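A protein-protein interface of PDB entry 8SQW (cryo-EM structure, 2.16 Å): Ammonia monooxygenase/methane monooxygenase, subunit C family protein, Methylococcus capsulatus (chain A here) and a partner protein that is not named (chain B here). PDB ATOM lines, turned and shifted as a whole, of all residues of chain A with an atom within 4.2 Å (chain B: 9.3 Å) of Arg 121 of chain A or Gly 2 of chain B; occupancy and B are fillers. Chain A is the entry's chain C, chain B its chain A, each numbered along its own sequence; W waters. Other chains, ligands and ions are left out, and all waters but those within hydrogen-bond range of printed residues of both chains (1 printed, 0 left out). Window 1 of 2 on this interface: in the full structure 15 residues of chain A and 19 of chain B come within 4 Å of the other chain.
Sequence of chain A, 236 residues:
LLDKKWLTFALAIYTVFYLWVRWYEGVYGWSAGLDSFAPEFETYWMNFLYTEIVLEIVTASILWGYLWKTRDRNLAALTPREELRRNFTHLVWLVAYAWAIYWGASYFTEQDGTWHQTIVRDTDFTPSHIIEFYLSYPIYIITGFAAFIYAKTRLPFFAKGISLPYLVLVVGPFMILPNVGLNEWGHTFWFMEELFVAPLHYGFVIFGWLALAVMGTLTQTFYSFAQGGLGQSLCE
Among the printed residues, pairs that only touch across the chains: Val 120 of chain A with Gly 2 of chain B (3.5 Å), Val 120 of chain A with Ile 119 of chain B (3.8 Å), Arg 121 of chain A with Gly 2 of chain B (3.9 Å) and Val 120 of chain A with Met 109 of chain B (3.97 Å).
Hydrophobic or aromatic side chains of chain B that line the printed part of chain A: Met 109 and Ile 119.
Of the 10 printed residues of chain A, 3 touch a printed residue of chain B.
Among the printed residues, 8 pairs touch across the chains.
Among the printed residues, no Asp or Glu carboxylate lies within 4 Å of a Lys or Arg side-chain nitrogen of the other chain.
The guanidinium group (NH2) of Arg 343 of chain B sits at hydrogen-bond distance from the backbone carbonyl oxygen (O) of Ser 5 of chain B, 3.3 Å away.
The side-chain sulfur (SD) of Met 109 of chain B sits close to the backbone NH (N) of Gly 60 of chain B, 3.6 Å away.
A ring nitrogen (NE2) of His 187 of chain A sits close to the guanidinium group (NH2) of Arg 121 of chain A.
The side-chain carboxylate (OE2) of Glu 194 of chain A lies within salt-bridge range of the guanidinium group (NH2) of Arg 121 of chain A.
Of the printed residues of chain B, Arg 121 of chain A touches Gly 2.
Gly 2 of chain B touches three residues of chain A.
Of chain B, only Gly 2, Met 109 and Ile 119 come within 4 Å of Val 120 of chain A.
Of the printed residues of chain B, Asp 122 of chain A touches His 1 (3.2 Å), Gly 2 (3.1 Å), Glu 3 (3.3 Å) and Ser 5 (3.0 Å).
Of the printed residues of chain A, Met 109 of chain B touches Val 120 (3.97 Å).
Of the printed residues of chain A, Ile 119 of chain B touches Val 120 (3.8 Å).
Of the printed residues of chain A, Ser 5 of chain B touches Asp 122.
Printed residues of chain A within 4 Å of Glu 3 of chain B: Asp 122 (3.3 Å).
Met 61 of chain B touches none of the printed residues of chain A.
Pro 117 of chain B touches none of the printed residues of chain A.
The nearest printed residue of chain A that does not touch Gly 2 of chain B is Ile 119 of chain A (6.8 Å).
The nearest printed residue of chain A that does not touch Ile 119 of chain B is Arg 121 of chain A (6.4 Å).
The side-chain carboxylate (OD1) of Asp 122 of chain A lies within hydrogen-bond range of the side-chain hydroxyl (OG) of Ser 5 of chain B (3.0 Å).
O of His 1 of chain B lies close to OD2 of Asp 122 of chain A, at 3.2 Å.
The side-chain carboxylate (OD1) of Asp 122 of chain A sits close to the backbone carbonyl oxygen (O) of Gly 2 of chain B, 3.2 Å away.
The side-chain carboxylate of Asp 122 of chain A lies close to the backbone carbonyl oxygen of Glu 3 of chain B, at 3.3 Å.
Water W1 lies within hydrogen-bond range of the backbone carbonyl oxygen of Gly 2 of chain B and the backbone carbonyl oxygen of Arg 121 of chain A.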
ATOM      1  N   HIS A 116     -11.724   7.033  14.771  1.00  0.00           N
ATOM      2  CA  HIS A 116     -10.924   6.466  15.883  1.00  0.00           C
ATOM      3  C   HIS A 116      -9.658   7.288  16.082  1.00  0.00           C
ATOM      4  O   HIS A 116      -9.316   7.587  17.239  1.00  0.00           O
ATOM      5  CB  HIS A 116     -10.514   5.030  15.538  1.00  0.00           C
ATOM      6  CG  HIS A 116     -11.646   4.115  15.187  1.00  0.00           C
ATOM      7  ND1 HIS A 116     -12.749   3.971  15.973  1.00  0.00           N
ATOM      8  CD2 HIS A 116     -11.825   3.278  14.124  1.00  0.00           C
ATOM      9  CE1 HIS A 116     -13.557   3.089  15.399  1.00  0.00           C
ATOM     10  NE2 HIS A 116     -13.039   2.654  14.274  1.00  0.00           N
ATOM     11  N   ILE A 119     -10.914   9.756  18.415  1.00  0.00           N
ATOM     12  CA  ILE A 119     -11.580   9.524  19.693  1.00  0.00           C
ATOM     13  C   ILE A 119     -11.045   8.231  20.294  1.00  0.00           C
ATOM     14  O   ILE A 119     -10.360   7.458  19.619  1.00  0.00           O
ATOM     15  CB  ILE A 119     -13.118   9.491  19.556  1.00  0.00           C
ATOM     16  CG1 ILE A 119     -13.579   8.371  18.620  1.00  0.00           C
ATOM     17  CG2 ILE A 119     -13.639  10.837  19.075  1.00  0.00           C
ATOM     18  CD1 ILE A 119     -13.964   7.089  19.327  1.00  0.00           C
ATOM     19  N   VAL A 120     -11.316   8.034  21.587  1.00  0.00           N
ATOM     20  CA  VAL A 120     -10.913   6.763  22.255  1.00  0.00           C
ATOM     21  C   VAL A 120     -12.116   5.824  22.161  1.00  0.00           C
ATOM     22  O   VAL A 120     -13.168   6.164  22.740  1.00  0.00           O
ATOM     23  CB  VAL A 120     -10.487   6.994  23.716  1.00  0.00           C
ATOM     24  CG1 VAL A 120     -10.691   5.749  24.566  1.00  0.00           C
ATOM     25  CG2 VAL A 120      -9.051   7.487  23.816  1.00  0.00           C
ATOM     26  N   ARG A 121     -11.974   4.707  21.444  1.00  0.00           N
ATOM     27  CA  ARG A 121     -13.132   3.799  21.237  1.00  0.00           C
ATOM     28  C   ARG A 121     -13.843   3.528  22.561  1.00  0.00           C
ATOM     29  O   ARG A 121     -13.178   3.553  23.618  1.00  0.00           O
ATOM     30  CB  ARG A 121     -12.692   2.442  20.694  1.00  0.00           C
ATOM     31  CG  ARG A 121     -12.287   2.458  19.231  1.00  0.00           C
ATOM     32  CD  ARG A 121     -11.260   1.356  19.164  1.00  0.00           C
ATOM     33  NE  ARG A 121     -11.653   0.270  18.279  1.00  0.00           N
ATOM     34  CZ  ARG A 121     -11.645   0.312  16.978  1.00  0.00           C
ATOM     35  NH1 ARG A 121     -12.618  -0.326  16.392  1.00  0.00           N
ATOM     36  NH2 ARG A 121     -10.701   0.940  16.299  1.00  0.00           N
ATOM     37  N   ASP A 122     -15.139   3.234  22.485  1.00  0.00           N
ATOM     38  CA  ASP A 122     -15.894   2.888  23.712  1.00  0.00           C
ATOM     39  C   ASP A 122     -16.598   1.547  23.502  1.00  0.00           C
ATOM     40  O   ASP A 122     -17.269   1.100  24.452  1.00  0.00           O
ATOM     41  CB  ASP A 122     -16.892   3.991  24.080  1.00  0.00           C
ATOM     42  CG  ASP A 122     -16.832   4.396  25.542  1.00  0.00           C
ATOM     43  OD1 ASP A 122     -15.729   4.335  26.122  1.00  0.00           O
ATOM     44  OD2 ASP A 122     -17.891   4.767  26.091  1.00  0.00           O
ATOM     45  N   THR A 123     -16.443   0.918  22.325  1.00  0.00           N
ATOM     46  CA  THR A 123     -17.213  -0.304  22.150  1.00  0.00           C
ATOM     47  C   THR A 123     -16.916  -0.854  20.764  1.00  0.00           C
ATOM     48  O   THR A 123     -16.216  -0.227  19.963  1.00  0.00           O
ATOM     49  CB  THR A 123     -18.717  -0.060  22.316  1.00  0.00           C
ATOM     50  OG1 THR A 123     -19.434  -1.268  22.038  1.00  0.00           O
ATOM     51  CG2 THR A 123     -19.181   1.029  21.365  1.00  0.00           C
ATOM     52  N   HIS A 129     -18.917   2.648  13.083  1.00  0.00           N
ATOM     53  CA  HIS A 129     -19.056   1.196  12.798  1.00  0.00           C
ATOM     54  C   HIS A 129     -20.528   0.925  12.486  1.00  0.00           C
ATOM     55  O   HIS A 129     -20.803   0.196  11.510  1.00  0.00           O
ATOM     56  CB  HIS A 129     -18.585   0.370  13.998  1.00  0.00           C
ATOM     57  CG  HIS A 129     -17.100   0.193  14.062  1.00  0.00           C
ATOM     58  ND1 HIS A 129     -16.462  -0.599  14.983  1.00  0.00           N
ATOM     59  CD2 HIS A 129     -16.142   0.749  13.269  1.00  0.00           C
ATOM     60  CE1 HIS A 129     -15.150  -0.537  14.766  1.00  0.00           C
ATOM     61  NE2 HIS A 129     -14.930   0.293  13.709  1.00  0.00           N
ATOM     62  N   ASN A 183     -11.192  -7.902  13.256  1.00  0.00           N
ATOM     63  CA  ASN A 183     -10.989  -6.472  13.609  1.00  0.00           C
ATOM     64  C   ASN A 183     -11.209  -6.292  15.113  1.00  0.00           C
ATOM     65  O   ASN A 183     -10.279  -5.816  15.793  1.00  0.00           O
ATOM     66  CB  ASN A 183     -11.919  -5.561  12.807  1.00  0.00           C
ATOM     67  CG  ASN A 183     -11.570  -4.094  12.938  1.00  0.00           C
ATOM     68  OD1 ASN A 183     -10.600  -3.627  12.356  1.00  0.00           O
ATOM     69  ND2 ASN A 183     -12.350  -3.352  13.702  1.00  0.00           N
ATOM     70  N   HIS A 187      -8.381  -5.783  18.218  1.00  0.00           N
ATOM     71  CA  HIS A 187      -8.366  -4.342  18.584  1.00  0.00           C
ATOM     72  C   HIS A 187      -8.297  -4.336  20.109  1.00  0.00           C
ATOM     73  O   HIS A 187      -7.383  -3.716  20.684  1.00  0.00           O
ATOM     74  CB  HIS A 187      -9.628  -3.631  18.041  1.00  0.00           C
ATOM     75  CG  HIS A 187      -9.360  -2.782  16.842  1.00  0.00           C
ATOM     76  ND1 HIS A 187      -8.140  -2.167  16.688  1.00  0.00           N
ATOM     77  CD2 HIS A 187     -10.020  -2.535  15.692  1.00  0.00           C
ATOM     78  CE1 HIS A 187      -8.072  -1.520  15.555  1.00  0.00           C
ATOM     79  NE2 HIS A 187      -9.195  -1.739  14.922  1.00  0.00           N
ATOM     80  N   GLU A 194      -3.890   2.419  17.754  1.00  0.00           N
ATOM     81  CA  GLU A 194      -4.906   2.696  16.704  1.00  0.00           C
ATOM     82  C   GLU A 194      -4.251   2.597  15.320  1.00  0.00           C
ATOM     83  O   GLU A 194      -4.801   3.184  14.368  1.00  0.00           O
ATOM     84  CB  GLU A 194      -5.529   4.078  16.920  1.00  0.00           C
ATOM     85  CG  GLU A 194      -6.857   4.031  17.652  1.00  0.00           C
ATOM     86  CD  GLU A 194      -7.848   3.025  17.092  1.00  0.00           C
ATOM     87  OE1 GLU A 194      -7.812   2.780  15.870  1.00  0.00           O
ATOM     88  OE2 GLU A 194      -8.658   2.496  17.875  1.00  0.00           O
ATOM     89  N   HIS B   1     -14.331  10.118  27.741  1.00  0.00           N
ATOM     90  CA  HIS B   1     -15.623   9.687  27.215  1.00  0.00           C
ATOM     91  C   HIS B   1     -15.312   8.258  26.792  1.00  0.00           C
ATOM     92  O   HIS B   1     -16.257   7.488  26.559  1.00  0.00           O
ATOM     93  CB  HIS B   1     -16.110  10.518  26.005  1.00  0.00           C
ATOM     94  CG  HIS B   1     -17.099  11.600  26.319  1.00  0.00           C
ATOM     95  ND1 HIS B   1     -16.982  12.322  27.475  1.00  0.00           N
ATOM     96  CD2 HIS B   1     -18.180  12.112  25.657  1.00  0.00           C
ATOM     97  CE1 HIS B   1     -17.969  13.192  27.547  1.00  0.00           C
ATOM     98  NE2 HIS B   1     -18.679  13.125  26.437  1.00  0.00           N
ATOM     99  N   GLY B   2     -14.009   7.944  26.721  1.00  0.00           N
ATOM    100  CA  GLY B   2     -13.555   6.593  26.345  1.00  0.00           C
ATOM    101  C   GLY B   2     -13.322   5.709  27.555  1.00  0.00           C
ATOM    102  O   GLY B   2     -12.803   4.596  27.370  1.00  0.00           O
ATOM    103  N   GLU B   3     -13.574   6.199  28.768  1.00  0.00           N
ATOM    104  CA  GLU B   3     -13.472   5.285  29.942  1.00  0.00           C
ATOM    105  C   GLU B   3     -14.894   4.796  30.265  1.00  0.00           C
ATOM    106  O   GLU B   3     -15.771   4.975  29.385  1.00  0.00           O
ATOM    107  CB  GLU B   3     -12.661   5.918  31.085  1.00  0.00           C
ATOM    108  CG  GLU B   3     -13.475   6.639  32.135  1.00  0.00           C
ATOM    109  CD  GLU B   3     -14.270   7.797  31.569  1.00  0.00           C
ATOM    110  OE1 GLU B   3     -13.662   8.837  31.275  1.00  0.00           O
ATOM    111  OE2 GLU B   3     -15.488   7.632  31.402  1.00  0.00           O
ATOM    112  N   LYS B   4     -15.117   4.182  31.433  1.00  0.00           N
ATOM    113  CA  LYS B   4     -16.440   3.567  31.762  1.00  0.00           C
ATOM    114  C   LYS B   4     -16.619   2.313  30.899  1.00  0.00           C
ATOM    115  O   LYS B   4     -17.637   1.638  31.080  1.00  0.00           O
ATOM    116  CB  LYS B   4     -17.618   4.524  31.540  1.00  0.00           C
ATOM    117  CG  LYS B   4     -17.834   5.577  32.613  1.00  0.00           C
ATOM    118  CD  LYS B   4     -18.482   6.834  32.077  1.00  0.00           C
ATOM    119  CE  LYS B   4     -19.720   7.243  32.844  1.00  0.00           C
ATOM    120  NZ  LYS B   4     -20.956   6.910  32.095  1.00  0.00           N
ATOM    121  N   SER B   5     -15.682   2.031  29.989  1.00  0.00           N
ATOM    122  CA  SER B   5     -15.733   0.835  29.111  1.00  0.00           C
ATOM    123  C   SER B   5     -14.487  -0.012  29.375  1.00  0.00           C
ATOM    124  O   SER B   5     -14.572  -1.233  29.195  1.00  0.00           O
ATOM    125  CB  SER B   5     -15.826   1.227  27.666  1.00  0.00           C
ATOM    126  OG  SER B   5     -16.994   1.994  27.430  1.00  0.00           O
ATOM    127  N   GLN B   6     -13.382   0.615  29.790  1.00  0.00           N
ATOM    128  CA  GLN B   6     -12.208  -0.162  30.143  1.00  0.00           C
ATOM    129  C   GLN B   6     -12.450  -0.948  31.427  1.00  0.00           C
ATOM    130  O   GLN B   6     -13.346  -0.642  32.219  1.00  0.00           O
ATOM    131  CB  GLN B   6     -10.992   0.749  30.304  1.00  0.00           C
ATOM    132  CG  GLN B   6     -10.988   1.941  29.370  1.00  0.00           C
ATOM    133  CD  GLN B   6      -9.757   2.806  29.543  1.00  0.00           C
ATOM    134  OE1 GLN B   6      -9.776   3.786  30.284  1.00  0.00           O
ATOM    135  NE2 GLN B   6      -8.680   2.448  28.857  1.00  0.00           N
ATOM    136  N   ALA B   7     -11.641  -1.985  31.617  1.00  0.00           N
ATOM    137  CA  ALA B   7     -11.774  -2.841  32.786  1.00  0.00           C
ATOM    138  C   ALA B   7     -11.592  -2.035  34.066  1.00  0.00           C
ATOM    139  O   ALA B   7     -10.705  -1.180  34.161  1.00  0.00           O
ATOM    140  CB  ALA B   7     -10.756  -3.978  32.722  1.00  0.00           C
ATOM    141  N   ARG B  11      -8.422   0.304  35.245  1.00  0.00           N
ATOM    142  CA  ARG B  11      -8.544   1.722  35.561  1.00  0.00           C
ATOM    143  C   ARG B  11      -8.098   2.010  36.987  1.00  0.00           C
ATOM    144  O   ARG B  11      -7.557   3.086  37.265  1.00  0.00           O
ATOM    145  CB  ARG B  11      -9.981   2.191  35.348  1.00  0.00           C
ATOM    146  CG  ARG B  11     -10.340   2.451  33.900  1.00  0.00           C
ATOM    147  CD  ARG B  11     -11.722   3.057  33.782  1.00  0.00           C
ATOM    148  NE  ARG B  11     -12.763   2.041  33.865  1.00  0.00           N
ATOM    149  CZ  ARG B  11     -13.902   2.187  34.525  1.00  0.00           C
ATOM    150  NH1 ARG B  11     -14.189   3.307  35.167  1.00  0.00           N
ATOM    151  NH2 ARG B  11     -14.777   1.186  34.543  1.00  0.00           N
ATOM    152  N   GLY B  60      -7.520  13.933  26.144  1.00  0.00           N
ATOM    153  CA  GLY B  60      -8.734  13.284  25.685  1.00  0.00           C
ATOM    154  C   GLY B  60      -9.792  14.296  25.302  1.00  0.00           C
ATOM    155  O   GLY B  60     -10.301  15.023  26.161  1.00  0.00           O
ATOM    156  N   MET B  61     -10.132  14.353  24.021  1.00  0.00           N
ATOM    157  CA  MET B  61     -11.009  15.399  23.514  1.00  0.00           C
ATOM    158  C   MET B  61     -11.544  14.970  22.157  1.00  0.00           C
ATOM    159  O   MET B  61     -10.924  14.149  21.469  1.00  0.00           O
ATOM    160  CB  MET B  61     -10.260  16.731  23.418  1.00  0.00           C
ATOM    161  CG  MET B  61      -9.465  16.907  22.147  1.00  0.00           C
ATOM    162  SD  MET B  61      -8.214  18.191  22.299  1.00  0.00           S
ATOM    163  CE  MET B  61      -8.935  19.169  23.605  1.00  0.00           C
ATOM    164  N   PRO B  62     -12.700  15.500  21.743  1.00  0.00           N
ATOM    165  CA  PRO B  62     -13.276  15.105  20.450  1.00  0.00           C
ATOM    166  C   PRO B  62     -12.672  15.857  19.277  1.00  0.00           C
ATOM    167  O   PRO B  62     -13.305  16.761  18.723  1.00  0.00           O
ATOM    168  CB  PRO B  62     -14.767  15.440  20.607  1.00  0.00           C
ATOM    169  CG  PRO B  62     -14.953  15.884  22.028  1.00  0.00           C
ATOM    170  CD  PRO B  62     -13.626  16.329  22.524  1.00  0.00           C
ATOM    171  N   HIS B 105     -15.716  17.785  26.791  1.00  0.00           N
ATOM    172  CA  HIS B 105     -15.261  17.024  27.949  1.00  0.00           C
ATOM    173  C   HIS B 105     -13.773  16.753  27.757  1.00  0.00           C
ATOM    174  O   HIS B 105     -13.384  15.885  26.972  1.00  0.00           O
ATOM    175  CB  HIS B 105     -16.061  15.733  28.096  1.00  0.00           C
ATOM    176  CG  HIS B 105     -16.192  15.266  29.509  1.00  0.00           C
ATOM    177  ND1 HIS B 105     -16.027  13.948  29.875  1.00  0.00           N
ATOM    178  CD2 HIS B 105     -16.471  15.941  30.651  1.00  0.00           C
ATOM    179  CE1 HIS B 105     -16.200  13.831  31.180  1.00  0.00           C
ATOM    180  NE2 HIS B 105     -16.468  15.026  31.673  1.00  0.00           N
ATOM    181  N   HIS B 107     -10.212  15.490  28.878  1.00  0.00           N
ATOM    182  CA  HIS B 107      -9.525  14.547  29.743  1.00  0.00           C
ATOM    183  C   HIS B 107      -8.021  14.725  29.601  1.00  0.00           C
ATOM    184  O   HIS B 107      -7.517  15.027  28.517  1.00  0.00           O
ATOM    185  CB  HIS B 107      -9.889  13.097  29.404  1.00  0.00           C
ATOM    186  CG  HIS B 107     -11.329  12.759  29.618  1.00  0.00           C
ATOM    187  ND1 HIS B 107     -11.765  11.990  30.673  1.00  0.00           N
ATOM    188  CD2 HIS B 107     -12.433  13.076  28.902  1.00  0.00           C
ATOM    189  CE1 HIS B 107     -13.075  11.850  30.602  1.00  0.00           C
ATOM    190  NE2 HIS B 107     -13.506  12.501  29.536  1.00  0.00           N
ATOM    191  N   MET B 109      -4.838  12.420  29.677  1.00  0.00           N
ATOM    192  CA  MET B 109      -4.629  10.995  29.517  1.00  0.00           C
ATOM    193  C   MET B 109      -3.159  10.676  29.281  1.00  0.00           C
ATOM    194  O   MET B 109      -2.369  11.514  28.843  1.00  0.00           O
ATOM    195  CB  MET B 109      -5.481  10.461  28.367  1.00  0.00           C
ATOM    196  CG  MET B 109      -5.360  11.272  27.097  1.00  0.00           C
ATOM    197  SD  MET B 109      -6.333  10.593  25.747  1.00  0.00           S
ATOM    198  CE  MET B 109      -5.972   8.851  25.917  1.00  0.00           C
ATOM    199  N   PRO B 117      -4.682   3.460  26.046  1.00  0.00           N
ATOM    200  CA  PRO B 117      -4.955   4.738  26.718  1.00  0.00           C
ATOM    201  C   PRO B 117      -5.299   4.610  28.194  1.00  0.00           C
ATOM    202  O   PRO B 117      -6.083   3.743  28.588  1.00  0.00           O
ATOM    203  CB  PRO B 117      -6.142   5.289  25.923  1.00  0.00           C
ATOM    204  CG  PRO B 117      -6.860   4.075  25.442  1.00  0.00           C
ATOM    205  CD  PRO B 117      -5.847   2.966  25.292  1.00  0.00           C
ATOM    206  N   ILE B 118      -4.719   5.479  29.017  1.00  0.00           N
ATOM    207  CA  ILE B 118      -5.058   5.573  30.434  1.00  0.00           C
ATOM    208  C   ILE B 118      -5.689   6.950  30.626  1.00  0.00           C
ATOM    209  O   ILE B 118      -5.004   7.969  30.704  1.00  0.00           O
ATOM    210  CB  ILE B 118      -3.842   5.360  31.331  1.00  0.00           C
ATOM    211  CG1 ILE B 118      -3.281   3.951  31.129  1.00  0.00           C
ATOM    212  CG2 ILE B 118      -4.207   5.581  32.791  1.00  0.00           C
ATOM    213  CD1 ILE B 118      -1.875   3.782  31.622  1.00  0.00           C
ATOM    214  N   ILE B 119      -7.019   6.976  30.699  1.00  0.00           N
ATOM    215  CA  ILE B 119      -7.747   8.236  30.708  1.00  0.00           C
ATOM    216  C   ILE B 119      -7.956   8.708  32.138  1.00  0.00           C
ATOM    217  O   ILE B 119      -8.480   7.971  32.985  1.00  0.00           O
ATOM    218  CB  ILE B 119      -9.086   8.090  29.969  1.00  0.00           C
ATOM    219  CG1 ILE B 119      -8.850   7.615  28.534  1.00  0.00           C
ATOM    220  CG2 ILE B 119      -9.846   9.399  29.976  1.00  0.00           C
ATOM    221  CD1 ILE B 119      -9.584   6.349  28.183  1.00  0.00           C
ATOM    222  N   GLY B 120      -7.551   9.944  32.416  1.00  0.00           N
ATOM    223  CA  GLY B 120      -7.771  10.552  33.705  1.00  0.00           C
ATOM    224  C   GLY B 120      -9.133  11.208  33.791  1.00  0.00           C
ATOM    225  O   GLY B 120      -9.980  11.052  32.907  1.00  0.00           O
ATOM    226  N   GLY B 122     -12.139  13.742  33.481  1.00  0.00           N
ATOM    227  CA  GLY B 122     -12.532  14.672  32.432  1.00  0.00           C
ATOM    228  C   GLY B 122     -13.405  15.777  32.988  1.00  0.00           C
ATOM    229  O   GLY B 122     -14.242  15.537  33.855  1.00  0.00           O
ATOM    230  N   TYR B 342     -19.746   4.923  36.432  1.00  0.00           N
ATOM    231  CA  TYR B 342     -18.476   4.673  35.765  1.00  0.00           C
ATOM    232  C   TYR B 342     -18.115   3.194  35.755  1.00  0.00           C
ATOM    233  O   TYR B 342     -16.967   2.844  35.471  1.00  0.00           O
ATOM    234  CB  TYR B 342     -17.370   5.501  36.419  1.00  0.00           C
ATOM    235  CG  TYR B 342     -17.335   6.918  35.907  1.00  0.00           C
ATOM    236  CD1 TYR B 342     -18.267   7.853  36.337  1.00  0.00           C
ATOM    237  CD2 TYR B 342     -16.380   7.322  34.985  1.00  0.00           C
ATOM    238  CE1 TYR B 342     -18.247   9.149  35.863  1.00  0.00           C
ATOM    239  CE2 TYR B 342     -16.351   8.616  34.507  1.00  0.00           C
ATOM    240  CZ  TYR B 342     -17.287   9.526  34.949  1.00  0.00           C
ATOM    241  OH  TYR B 342     -17.259  10.817  34.478  1.00  0.00           O
ATOM    242  N   ARG B 343     -19.112   2.341  36.023  1.00  0.00           N
ATOM    243  CA  ARG B 343     -18.932   0.864  35.939  1.00  0.00           C
ATOM    244  C   ARG B 343     -17.729   0.379  36.753  1.00  0.00           C
ATOM    245  O   ARG B 343     -16.984  -0.483  36.244  1.00  0.00           O
ATOM    246  CB  ARG B 343     -18.863   0.446  34.465  1.00  0.00           C
ATOM    247  CG  ARG B 343     -20.192   0.575  33.735  1.00  0.00           C
ATOM    248  CD  ARG B 343     -20.335  -0.521  32.703  1.00  0.00           C
ATOM    249  NE  ARG B 343     -19.081  -0.598  31.976  1.00  0.00           N
ATOM    250  CZ  ARG B 343     -18.506  -1.702  31.522  1.00  0.00           C
ATOM    251  NH1 ARG B 343     -19.079  -2.881  31.686  1.00  0.00           N
ATOM    252  NH2 ARG B 343     -17.356  -1.607  30.883  1.00  0.00           N
HETATM  253  O   HOH W   1     -12.022   2.367  26.143  1.00  0.00           O
